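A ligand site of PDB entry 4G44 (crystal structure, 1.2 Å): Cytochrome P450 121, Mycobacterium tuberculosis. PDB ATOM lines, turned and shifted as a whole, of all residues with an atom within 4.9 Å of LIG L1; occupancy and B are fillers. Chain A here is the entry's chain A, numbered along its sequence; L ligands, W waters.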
ATOM      1  N   LEU A  55     -19.657 -17.205  23.461  1.00  0.00           N
ATOM      2  CA  LEU A  55     -18.859 -17.118  22.287  1.00  0.00           C
ATOM      3  C   LEU A  55     -19.410 -16.145  21.160  1.00  0.00           C
ATOM      4  O   LEU A  55     -18.662 -15.695  20.367  1.00  0.00           O
ATOM      5  CB  LEU A  55     -18.672 -18.497  21.637  1.00  0.00           C
ATOM      6  CG  LEU A  55     -17.811 -19.461  22.510  1.00  0.00           C
ATOM      7  CD1 LEU A  55     -17.790 -20.847  21.852  1.00  0.00           C
ATOM      8  CD2 LEU A  55     -16.397 -18.927  22.698  1.00  0.00           C
ATOM      9  N   MET A  62     -11.594 -12.109  23.530  1.00  0.00           N
ATOM     10  CA  MET A  62     -10.378 -12.901  23.532  1.00  0.00           C
ATOM     11  C   MET A  62      -9.213 -11.977  23.727  1.00  0.00           C
ATOM     12  O   MET A  62      -8.308 -12.263  24.563  1.00  0.00           O
ATOM     13  CB  MET A  62     -10.219 -13.627  22.153  1.00  0.00           C
ATOM     14  CG  MET A  62      -8.634 -14.252  21.925  1.00  0.00           C
ATOM     15  SD  MET A  62      -8.574 -15.007  20.329  1.00  0.00           S
ATOM     16  CE  MET A  62      -9.617 -16.403  20.537  1.00  0.00           C
ATOM     17  N   MET A  86      -5.525 -13.285  14.887  1.00  0.00           N
ATOM     18  CA  MET A  86      -6.394 -13.147  13.719  1.00  0.00           C
ATOM     19  C   MET A  86      -6.873 -11.765  13.569  1.00  0.00           C
ATOM     20  O   MET A  86      -7.044 -11.297  12.388  1.00  0.00           O
ATOM     21  CB  MET A  86      -7.632 -14.062  13.855  1.00  0.00           C
ATOM     22  CG  MET A  86      -7.401 -15.457  13.296  1.00  0.00           C
ATOM     23  SD  MET A  86      -7.023 -15.633  11.536  1.00  0.00           S
ATOM     24  CE  MET A  86      -8.602 -15.743  10.792  1.00  0.00           C
ATOM     25  N   ILE A 102      -5.260 -21.813   3.454  1.00  0.00           N
ATOM     26  CA  ILE A 102      -5.341 -22.966   4.367  1.00  0.00           C
ATOM     27  C   ILE A 102      -6.593 -23.766   4.137  1.00  0.00           C
ATOM     28  O   ILE A 102      -6.938 -24.634   4.992  1.00  0.00           O
ATOM     29  CB  ILE A 102      -5.154 -22.520   5.846  1.00  0.00           C
ATOM     30  CG1 ILE A 102      -6.323 -21.683   6.362  1.00  0.00           C
ATOM     31  CG2 ILE A 102      -3.808 -21.812   6.010  1.00  0.00           C
ATOM     32  CD1 ILE A 102      -6.359 -21.460   7.854  1.00  0.00           C
ATOM     33  N   HIS A 146       1.177 -29.564   7.260  1.00  0.00           N
ATOM     34  CA  HIS A 146       1.398 -28.166   7.488  1.00  0.00           C
ATOM     35  C   HIS A 146       2.606 -27.663   6.779  1.00  0.00           C
ATOM     36  O   HIS A 146       2.618 -26.467   6.365  1.00  0.00           O
ATOM     37  CB  HIS A 146       1.313 -27.799   8.982  1.00  0.00           C
ATOM     38  CG  HIS A 146      -0.095 -27.843   9.449  1.00  0.00           C
ATOM     39  ND1 HIS A 146      -0.786 -28.999   9.722  1.00  0.00           N
ATOM     40  CD2 HIS A 146      -1.018 -26.868   9.623  1.00  0.00           C
ATOM     41  CE1 HIS A 146      -2.047 -28.711  10.062  1.00  0.00           C
ATOM     42  NE2 HIS A 146      -2.212 -27.396  10.016  1.00  0.00           N
ATOM     43  N   PHE A 230       0.361 -20.330  12.686  1.00  0.00           N
ATOM     44  CA  PHE A 230      -0.448 -21.263  11.918  1.00  0.00           C
ATOM     45  C   PHE A 230       0.208 -22.620  11.878  1.00  0.00           C
ATOM     46  O   PHE A 230      -0.585 -23.640  11.992  1.00  0.00           O
ATOM     47  CB  PHE A 230      -0.776 -20.730  10.485  1.00  0.00           C
ATOM     48  CG  PHE A 230      -1.954 -19.748  10.502  1.00  0.00           C
ATOM     49  CD1 PHE A 230      -1.940 -18.605  11.308  1.00  0.00           C
ATOM     50  CD2 PHE A 230      -3.095 -20.005   9.838  1.00  0.00           C
ATOM     51  CE1 PHE A 230      -3.027 -17.729  11.338  1.00  0.00           C
ATOM     52  CE2 PHE A 230      -4.175 -19.101   9.852  1.00  0.00           C
ATOM     53  CZ  PHE A 230      -4.097 -17.974  10.633  1.00  0.00           C
ATOM     54  N   ALA A 233      -0.446 -23.967  15.766  1.00  0.00           N
ATOM     55  CA  ALA A 233      -1.822 -24.222  16.121  1.00  0.00           C
ATOM     56  C   ALA A 233      -2.425 -25.280  15.223  1.00  0.00           C
ATOM     57  O   ALA A 233      -3.192 -26.146  15.665  1.00  0.00           O
ATOM     58  CB  ALA A 233      -2.642 -22.900  16.056  1.00  0.00           C
ATOM     59  N   GLY A 234      -2.095 -25.288  13.928  1.00  0.00           N
ATOM     60  CA  GLY A 234      -2.653 -26.246  13.062  1.00  0.00           C
ATOM     61  C   GLY A 234      -2.082 -27.672  13.371  1.00  0.00           C
ATOM     62  O   GLY A 234      -2.892 -28.646  13.403  1.00  0.00           O
ATOM     63  N   SER A 237      -3.387 -28.939  16.739  1.00  0.00           N
ATOM     64  CA  SER A 237      -4.793 -29.164  16.793  1.00  0.00           C
ATOM     65  C   SER A 237      -5.204 -30.399  15.988  1.00  0.00           C
ATOM     66  O   SER A 237      -5.982 -31.253  16.454  1.00  0.00           O
ATOM     67  CB  SER A 237      -5.594 -27.996  16.296  1.00  0.00           C
ATOM     68  OG  SER A 237      -5.346 -26.828  17.115  1.00  0.00           O
ATOM     69  N   THR A 238      -4.639 -30.549  14.777  1.00  0.00           N
ATOM     70  CA  THR A 238      -4.967 -31.694  13.913  1.00  0.00           C
ATOM     71  C   THR A 238      -4.283 -32.952  14.439  1.00  0.00           C
ATOM     72  O   THR A 238      -4.975 -34.018  14.439  1.00  0.00           O
ATOM     73  CB  THR A 238      -4.545 -31.420  12.450  1.00  0.00           C
ATOM     74  OG1 THR A 238      -3.187 -31.165  12.349  1.00  0.00           O
ATOM     75  CG2 THR A 238      -5.352 -30.272  11.806  1.00  0.00           C
ATOM     76  N   PHE A 241      -6.312 -33.925  17.674  1.00  0.00           N
ATOM     77  CA  PHE A 241      -7.654 -34.373  17.346  1.00  0.00           C
ATOM     78  C   PHE A 241      -7.612 -35.762  16.689  1.00  0.00           C
ATOM     79  O   PHE A 241      -8.343 -36.670  17.151  1.00  0.00           O
ATOM     80  CB  PHE A 241      -8.386 -33.391  16.441  1.00  0.00           C
ATOM     81  CG  PHE A 241      -9.693 -33.994  15.966  1.00  0.00           C
ATOM     82  CD1 PHE A 241     -10.665 -34.361  16.855  1.00  0.00           C
ATOM     83  CD2 PHE A 241      -9.842 -34.324  14.607  1.00  0.00           C
ATOM     84  CE1 PHE A 241     -11.805 -35.061  16.447  1.00  0.00           C
ATOM     85  CE2 PHE A 241     -11.011 -35.014  14.177  1.00  0.00           C
ATOM     86  CZ  PHE A 241     -11.943 -35.372  15.082  1.00  0.00           C
ATOM     87  N   LEU A 274     -15.480 -35.262  16.080  1.00  0.00           N
ATOM     88  CA  LEU A 274     -15.252 -33.840  16.508  1.00  0.00           C
ATOM     89  C   LEU A 274     -16.131 -33.523  17.621  1.00  0.00           C
ATOM     90  O   LEU A 274     -15.725 -32.934  18.661  1.00  0.00           O
ATOM     91  CB  LEU A 274     -15.502 -32.883  15.327  1.00  0.00           C
ATOM     92  CG  LEU A 274     -14.354 -32.860  14.318  1.00  0.00           C
ATOM     93  CD1 LEU A 274     -14.853 -32.267  12.982  1.00  0.00           C
ATOM     94  CD2 LEU A 274     -13.155 -32.032  14.869  1.00  0.00           C
ATOM     95  N   PHE A 280      -9.444 -30.489  23.708  1.00  0.00           N
ATOM     96  CA  PHE A 280      -9.132 -29.194  24.410  1.00  0.00           C
ATOM     97  C   PHE A 280      -9.125 -29.418  25.883  1.00  0.00           C
ATOM     98  O   PHE A 280     -10.116 -29.795  26.478  1.00  0.00           O
ATOM     99  CB  PHE A 280     -10.153 -28.104  24.005  1.00  0.00           C
ATOM    100  CG  PHE A 280      -9.754 -27.420  22.759  1.00  0.00           C
ATOM    101  CD1 PHE A 280      -9.767 -28.109  21.566  1.00  0.00           C
ATOM    102  CD2 PHE A 280      -9.293 -26.117  22.744  1.00  0.00           C
ATOM    103  CE1 PHE A 280      -9.312 -27.427  20.352  1.00  0.00           C
ATOM    104  CE2 PHE A 280      -8.867 -25.492  21.555  1.00  0.00           C
ATOM    105  CZ  PHE A 280      -8.906 -26.165  20.426  1.00  0.00           C
ATOM    106  N   LEU A 284     -12.244 -22.399  26.646  1.00  0.00           N
ATOM    107  CA  LEU A 284     -11.774 -21.261  25.902  1.00  0.00           C
ATOM    108  C   LEU A 284     -11.914 -20.003  26.754  1.00  0.00           C
ATOM    109  O   LEU A 284     -13.000 -19.717  27.239  1.00  0.00           O
ATOM    110  CB  LEU A 284     -12.593 -21.025  24.613  1.00  0.00           C
ATOM    111  CG  LEU A 284     -12.632 -22.268  23.660  1.00  0.00           C
ATOM    112  CD1 LEU A 284     -13.487 -21.891  22.465  1.00  0.00           C
ATOM    113  CD2 LEU A 284     -11.220 -22.770  23.290  1.00  0.00           C
ATOM    114  N   ARG A 286     -12.141 -16.012  27.886  1.00  0.00           N
ATOM    115  CA  ARG A 286     -12.607 -14.701  27.486  1.00  0.00           C
ATOM    116  C   ARG A 286     -12.595 -13.778  28.702  1.00  0.00           C
ATOM    117  O   ARG A 286     -12.836 -14.253  29.800  1.00  0.00           O
ATOM    118  CB  ARG A 286     -14.055 -14.775  26.958  1.00  0.00           C
ATOM    119  CG  ARG A 286     -14.260 -15.616  25.697  1.00  0.00           C
ATOM    120  CD  ARG A 286     -13.629 -14.983  24.534  1.00  0.00           C
ATOM    121  NE  ARG A 286     -13.972 -15.646  23.234  1.00  0.00           N
ATOM    122  CZ  ARG A 286     -13.253 -16.604  22.677  1.00  0.00           C
ATOM    123  NH1 ARG A 286     -12.164 -17.139  23.193  1.00  0.00           N
ATOM    124  NH2 ARG A 286     -13.676 -17.036  21.442  1.00  0.00           N
ATOM    125  N   LEU A 309     -15.860 -26.647  26.133  1.00  0.00           N
ATOM    126  CA  LEU A 309     -16.408 -27.183  24.856  1.00  0.00           C
ATOM    127  C   LEU A 309     -17.109 -28.482  25.085  1.00  0.00           C
ATOM    128  O   LEU A 309     -18.222 -28.678  24.450  1.00  0.00           O
ATOM    129  CB  LEU A 309     -15.297 -27.317  23.847  1.00  0.00           C
ATOM    130  CG  LEU A 309     -14.624 -25.999  23.434  1.00  0.00           C
ATOM    131  CD1 LEU A 309     -13.592 -26.275  22.344  1.00  0.00           C
ATOM    132  CD2 LEU A 309     -15.598 -24.926  22.989  1.00  0.00           C
ATOM    133  N   LEU A 336     -19.432 -27.351  18.990  1.00  0.00           N
ATOM    134  CA  LEU A 336     -18.493 -26.247  19.224  1.00  0.00           C
ATOM    135  C   LEU A 336     -17.080 -26.701  19.090  1.00  0.00           C
ATOM    136  O   LEU A 336     -16.163 -25.984  19.640  1.00  0.00           O
ATOM    137  CB  LEU A 336     -18.768 -25.605  20.577  1.00  0.00           C
ATOM    138  CG  LEU A 336     -20.148 -25.085  20.804  1.00  0.00           C
ATOM    139  CD1 LEU A 336     -20.170 -24.196  22.077  1.00  0.00           C
ATOM    140  CD2 LEU A 336     -20.823 -24.386  19.652  1.00  0.00           C
ATOM    141  N   ALA A 337     -16.769 -27.817  18.443  1.00  0.00           N
ATOM    142  CA  ALA A 337     -15.343 -28.237  18.388  1.00  0.00           C
ATOM    143  C   ALA A 337     -14.406 -27.256  17.745  1.00  0.00           C
ATOM    144  O   ALA A 337     -13.213 -27.262  18.034  1.00  0.00           O
ATOM    145  CB  ALA A 337     -15.178 -29.590  17.649  1.00  0.00           C
ATOM    146  N   PHE A 338     -14.911 -26.403  16.820  1.00  0.00           N
ATOM    147  CA  PHE A 338     -14.150 -25.381  16.159  1.00  0.00           C
ATOM    148  C   PHE A 338     -14.491 -23.986  16.740  1.00  0.00           C
ATOM    149  O   PHE A 338     -14.138 -22.944  16.079  1.00  0.00           O
ATOM    150  CB  PHE A 338     -14.412 -25.403  14.626  1.00  0.00           C
ATOM    151  CG  PHE A 338     -13.927 -26.654  13.960  1.00  0.00           C
ATOM    152  CD1 PHE A 338     -12.571 -26.943  13.970  1.00  0.00           C
ATOM    153  CD2 PHE A 338     -14.798 -27.514  13.289  1.00  0.00           C
ATOM    154  CE1 PHE A 338     -12.080 -28.104  13.297  1.00  0.00           C
ATOM    155  CE2 PHE A 338     -14.300 -28.603  12.643  1.00  0.00           C
ATOM    156  CZ  PHE A 338     -12.961 -28.924  12.618  1.00  0.00           C
ATOM    157  N   GLY A 339     -15.109 -23.929  17.868  1.00  0.00           N
ATOM    158  CA  GLY A 339     -15.520 -22.641  18.438  1.00  0.00           C
ATOM    159  C   GLY A 339     -16.818 -22.163  17.761  1.00  0.00           C
ATOM    160  O   GLY A 339     -17.604 -22.955  17.151  1.00  0.00           O
ATOM    161  N   GLN A 342     -16.986 -14.829  16.427  1.00  0.00           N
ATOM    162  CA  GLN A 342     -15.899 -14.045  15.861  1.00  0.00           C
ATOM    163  C   GLN A 342     -14.625 -14.878  15.637  1.00  0.00           C
ATOM    164  O   GLN A 342     -13.910 -14.619  14.672  1.00  0.00           O
ATOM    165  CB  GLN A 342     -15.596 -12.859  16.841  1.00  0.00           C
ATOM    166  CG  GLN A 342     -14.437 -11.914  16.359  1.00  0.00           C
ATOM    167  CD  GLN A 342     -14.750 -11.094  15.165  1.00  0.00           C
ATOM    168  OE1 GLN A 342     -13.831 -10.429  14.585  1.00  0.00           O
ATOM    169  NE2 GLN A 342     -15.975 -10.948  14.839  1.00  0.00           N
ATOM    170  N   HIS A 343     -14.346 -15.795  16.580  1.00  0.00           N
ATOM    171  CA  HIS A 343     -13.076 -16.514  16.535  1.00  0.00           C
ATOM    172  C   HIS A 343     -13.206 -17.929  16.024  1.00  0.00           C
ATOM    173  O   HIS A 343     -12.280 -18.774  16.263  1.00  0.00           O
ATOM    174  CB  HIS A 343     -12.375 -16.444  17.912  1.00  0.00           C
ATOM    175  CG  HIS A 343     -12.067 -15.031  18.298  1.00  0.00           C
ATOM    176  ND1 HIS A 343     -11.022 -14.394  17.745  1.00  0.00           N
ATOM    177  CD2 HIS A 343     -12.706 -14.129  19.127  1.00  0.00           C
ATOM    178  CE1 HIS A 343     -10.945 -13.138  18.219  1.00  0.00           C
ATOM    179  NE2 HIS A 343     -11.970 -12.962  19.051  1.00  0.00           N
ATOM    180  N   PHE A 344     -14.290 -18.265  15.308  1.00  0.00           N
ATOM    181  CA  PHE A 344     -14.471 -19.619  14.761  1.00  0.00           C
ATOM    182  C   PHE A 344     -13.220 -20.010  13.956  1.00  0.00           C
ATOM    183  O   PHE A 344     -12.646 -19.234  13.186  1.00  0.00           O
ATOM    184  CB  PHE A 344     -15.647 -19.583  13.796  1.00  0.00           C
ATOM    185  CG  PHE A 344     -15.956 -20.930  13.224  1.00  0.00           C
ATOM    186  CD1 PHE A 344     -16.683 -21.812  13.909  1.00  0.00           C
ATOM    187  CD2 PHE A 344     -15.493 -21.257  11.965  1.00  0.00           C
ATOM    188  CE1 PHE A 344     -16.982 -23.123  13.407  1.00  0.00           C
ATOM    189  CE2 PHE A 344     -15.743 -22.583  11.456  1.00  0.00           C
ATOM    190  CZ  PHE A 344     -16.437 -23.475  12.171  1.00  0.00           C
ATOM    191  N   CYS A 345     -12.760 -21.258  14.129  1.00  0.00           N
ATOM    192  CA  CYS A 345     -11.497 -21.752  13.571  1.00  0.00           C
ATOM    193  C   CYS A 345     -11.434 -21.558  12.039  1.00  0.00           C
ATOM    194  O   CYS A 345     -12.231 -22.125  11.316  1.00  0.00           O
ATOM    195  CB  CYS A 345     -11.371 -23.248  13.867  1.00  0.00           C
ATOM    196  SG  CYS A 345      -9.797 -23.902  13.235  1.00  0.00           S
ATOM    197  N   PRO A 346     -10.447 -20.874  11.518  1.00  0.00           N
ATOM    198  CA  PRO A 346     -10.307 -20.710  10.054  1.00  0.00           C
ATOM    199  C   PRO A 346      -9.683 -21.935   9.460  1.00  0.00           C
ATOM    200  O   PRO A 346      -9.725 -22.095   8.191  1.00  0.00           O
ATOM    201  CB  PRO A 346      -9.336 -19.505   9.904  1.00  0.00           C
ATOM    202  CG  PRO A 346      -8.503 -19.620  11.085  1.00  0.00           C
ATOM    203  CD  PRO A 346      -9.458 -20.048  12.251  1.00  0.00           C
ATOM    204  N   GLY A 347      -9.200 -22.887  10.247  1.00  0.00           N
ATOM    205  CA  GLY A 347      -8.684 -24.182   9.699  1.00  0.00           C
ATOM    206  C   GLY A 347      -9.672 -25.284   9.722  1.00  0.00           C
ATOM    207  O   GLY A 347      -9.229 -26.429   9.499  1.00  0.00           O
ATOM    208  N   LEU A 350      -9.658 -27.738   6.699  1.00  0.00           N
ATOM    209  CA  LEU A 350      -8.430 -28.425   6.649  1.00  0.00           C
ATOM    210  C   LEU A 350      -8.386 -29.555   7.737  1.00  0.00           C
ATOM    211  O   LEU A 350      -7.857 -30.674   7.532  1.00  0.00           O
ATOM    212  CB  LEU A 350      -7.246 -27.522   6.708  1.00  0.00           C
ATOM    213  CG  LEU A 350      -5.880 -28.106   6.544  1.00  0.00           C
ATOM    214  CD1 LEU A 350      -5.680 -28.628   5.107  1.00  0.00           C
ATOM    215  CD2 LEU A 350      -4.841 -27.069   6.773  1.00  0.00           C
ATOM    216  N   GLY A 351      -8.786 -29.205   8.959  1.00  0.00           N
ATOM    217  CA  GLY A 351      -8.786 -30.152  10.025  1.00  0.00           C
ATOM    218  C   GLY A 351      -9.701 -31.310   9.784  1.00  0.00           C
ATOM    219  O   GLY A 351      -9.328 -32.496  10.021  1.00  0.00           O
HETATM  220  C1  LIG L   1      -9.360 -21.038  16.393  1.00  0.00           C
HETATM  221  C2  LIG L   1     -10.165 -25.767  17.053  1.00  0.00           C
HETATM  222  C3  LIG L   1      -7.394 -26.812  13.234  1.00  0.00           C
HETATM  223  C4  LIG L   1      -5.887 -22.193  13.150  1.00  0.00           C
HETATM  224  C5  LIG L   1      -9.865 -22.265  16.854  1.00  0.00           C
HETATM  225  C6  LIG L   1     -10.822 -22.367  17.930  1.00  0.00           C
HETATM  226  C7  LIG L   1     -11.055 -23.709  18.179  1.00  0.00           C
HETATM  227  C8  LIG L   1     -10.205 -24.406  17.202  1.00  0.00           C
HETATM  228  C9  LIG L   1     -11.882 -24.336  19.227  1.00  0.00           C
HETATM  229  C10 LIG L   1     -11.483 -21.221  18.639  1.00  0.00           C
HETATM  230  C11 LIG L   1     -10.631 -20.659  19.751  1.00  0.00           C
HETATM  231  C12 LIG L   1     -11.368 -19.603  20.537  1.00  0.00           C
HETATM  232  O1  LIG L   1     -12.446 -19.109  20.170  1.00  0.00           O
HETATM  233  O2  LIG L   1     -10.817 -19.187  21.689  1.00  0.00           O
HETATM  234  C13 LIG L   1      -9.458 -26.495  16.048  1.00  0.00           C
HETATM  235  C14 LIG L   1      -9.581 -27.886  15.878  1.00  0.00           C
HETATM  236  C15 LIG L   1      -8.754 -28.169  14.763  1.00  0.00           C
HETATM  237  C16 LIG L   1      -8.188 -26.963  14.355  1.00  0.00           C
HETATM  238  C17 LIG L   1     -10.392 -28.815  16.663  1.00  0.00           C
HETATM  239  C18 LIG L   1      -8.497 -29.492  14.115  1.00  0.00           C
HETATM  240  C19 LIG L   1      -9.272 -30.602  14.107  1.00  0.00           C
HETATM  241  C20 LIG L   1      -6.782 -25.639  12.841  1.00  0.00           C
HETATM  242  C21 LIG L   1      -5.884 -25.475  11.710  1.00  0.00           C
HETATM  243  C22 LIG L   1      -5.386 -24.183  11.734  1.00  0.00           C
HETATM  244  C23 LIG L   1      -6.092 -23.522  12.784  1.00  0.00           C
HETATM  245  C24 LIG L   1      -5.551 -26.559  10.698  1.00  0.00           C
HETATM  246  C25 LIG L   1      -4.424 -23.547  10.805  1.00  0.00           C
HETATM  247  C26 LIG L   1      -3.643 -24.135   9.872  1.00  0.00           C
HETATM  248  C27 LIG L   1      -6.711 -21.442  14.071  1.00  0.00           C
HETATM  249  C28 LIG L   1      -6.622 -19.998  14.252  1.00  0.00           C
HETATM  250  C29 LIG L   1      -7.647 -19.683  15.186  1.00  0.00           C
HETATM  251  C30 LIG L   1      -8.245 -20.954  15.503  1.00  0.00           C
HETATM  252  C31 LIG L   1      -5.657 -19.063  13.556  1.00  0.00           C
HETATM  253  C32 LIG L   1      -8.040 -18.269  15.712  1.00  0.00           C
HETATM  254  C33 LIG L   1      -9.143 -17.657  15.004  1.00  0.00           C
HETATM  255  C34 LIG L   1      -9.631 -16.246  15.536  1.00  0.00           C
HETATM  256  O3  LIG L   1     -10.417 -15.678  14.822  1.00  0.00           O
HETATM  257  O4  LIG L   1      -9.170 -15.944  16.545  1.00  0.00           O
HETATM  258  N1  LIG L   1      -9.481 -23.522  16.400  1.00  0.00           N
HETATM  259  N2  LIG L   1      -8.583 -25.940  15.168  1.00  0.00           N
HETATM  260  N3  LIG L   1      -6.939 -24.413  13.496  1.00  0.00           N
HETATM  261  N4  LIG L   1      -7.715 -21.990  14.787  1.00  0.00           N
HETATM  262 FE1  LIG L   1      -8.239 -23.942  14.921  1.00  0.00          FE
HETATM  263  C1  LG2 L   2      -6.065 -21.902  17.358  1.00  0.00           C
HETATM  264  C2  LG2 L   2      -6.612 -23.172  17.449  1.00  0.00           C
HETATM  265  N1  LG2 L   2      -6.539 -24.066  16.306  1.00  0.00           N
HETATM  266  C3  LG2 L   2      -7.358 -23.537  18.582  1.00  0.00           C
HETATM  267  C4  LG2 L   2      -7.440 -22.669  19.654  1.00  0.00           C
HETATM  268  C5  LG2 L   2      -6.828 -21.397  19.644  1.00  0.00           C
HETATM  269  C6  LG2 L   2      -6.160 -21.029  18.478  1.00  0.00           C
HETATM  270  C7  LG2 L   2      -5.641 -19.635  18.532  1.00  0.00           C
HETATM  271  N2  LG2 L   2      -4.653 -19.255  17.571  1.00  0.00           N
HETATM  272  N3  LG2 L   2      -3.565 -19.927  17.436  1.00  0.00           N
HETATM  273  C8  LG2 L   2      -2.909 -19.315  16.425  1.00  0.00           C
HETATM  274  N4  LG2 L   2      -3.508 -18.107  16.126  1.00  0.00           N
HETATM  275  C9  LG2 L   2      -4.622 -18.095  16.829  1.00  0.00           C
HETATM  276  O   HOH W   1     -14.730 -19.435  18.790  1.00  0.00           O
HETATM  277  O   HOH W   2      -6.564 -15.100  17.074  1.00  0.00           O
HETATM  278  O   HOH W   3     -11.312 -13.279  14.287  1.00  0.00           O
HETATM  279  O   HOH W   4     -11.473 -16.643  12.668  1.00  0.00           O
HETATM  280  O   HOH W   5      -8.419 -19.716  22.759  1.00  0.00           O
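The guanidinium group (NH2) of Arg 286 is in salt-bridge range of an oxygen (O1) of LIG L1 (2.7 Å). An oxygen (O4) of LIG L1 lies within hydrogen-bond range of a ring nitrogen (ND1) of His 343, 2.7 Å away. The side-chain hydroxyl of Ser 237 sits close to a nitrogen (N1) of LG2 L2 (3.1 Å). An iron atom (FE1) of LIG L1 is bound by the side-chain sulfur of Cys 345 (2.3 Å).
An iron atom (FE1) of LIG L1 is bound by a nitrogen (N1) of LG2 L2.
OG1 of Thr 238 sits at hydrogen-bond distance from O of Gly 234, 2.7 Å away. The backbone NH of Cys 345 lies within hydrogen-bond range of the backbone carbonyl oxygen of Phe 338, at 2.9 Å. The side-chain sulfur (SG) of Cys 345 sits close to the backbone NH (N) of Gly 347, 3.2 Å away. A ring nitrogen (ND1) of His 343 is in hydrogen-bond range of the side-chain sulfur (SD) of Met 62, 3.6 Å away. OG of Ser 237 lies within hydrogen-bond range of O of Ala 233, at 2.7 Å.
CE of Met 62 touches O2 of LIG L1 (3.2 Å). Met 86 touches LIG L1. His 146 touches LIG L1 (NE2 to C24, 3.5 Å). Phe 230 touches LIG L1. Gly 234 touches LIG L1. CB of Ser 237 touches C16 of LIG L1 (3.4 Å). CG2 of Thr 238 touches C24 of LIG L1, at 3.9 Å. Phe 241 touches LIG L1. CZ of Phe 280 touches C2 of LIG L1 (3.6 Å). Leu 284 touches LIG L1 (CD1 to C12, 3.7 Å). Ala 337 touches LIG L1. CE1 of Phe 338 touches C14 of LIG L1, 3.6 Å away. Gly 339 touches LIG L1. Gln 342 touches LIG L1. Pro 346 touches LIG L1 (CD to C29, 3.5 Å). CA of Gly 347 touches C21 of LIG L1, at 3.7 Å. Hydrophobic or aromatic side chains within 4 Å of LIG L1: Met 62, Met 86, His 146, Phe 230, Phe 241, Phe 280, Leu 284, Phe 338, His 343 and Pro 346. Of the 28 residues printed, 19 come within 4 Å of LIG L1.
Water W4 lies within hydrogen-bond range of O3 of LIG L1 (2.6 Å) and O of Phe 344 (2.9 Å). Water W3 lies within hydrogen-bond range of O3 of LIG L1 and O of Gln 342. Water W2 lies within hydrogen-bond range of an oxygen (O4) of LIG L1 (2.8 Å) and the backbone NH (N) of Met 86 (3.0 Å).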
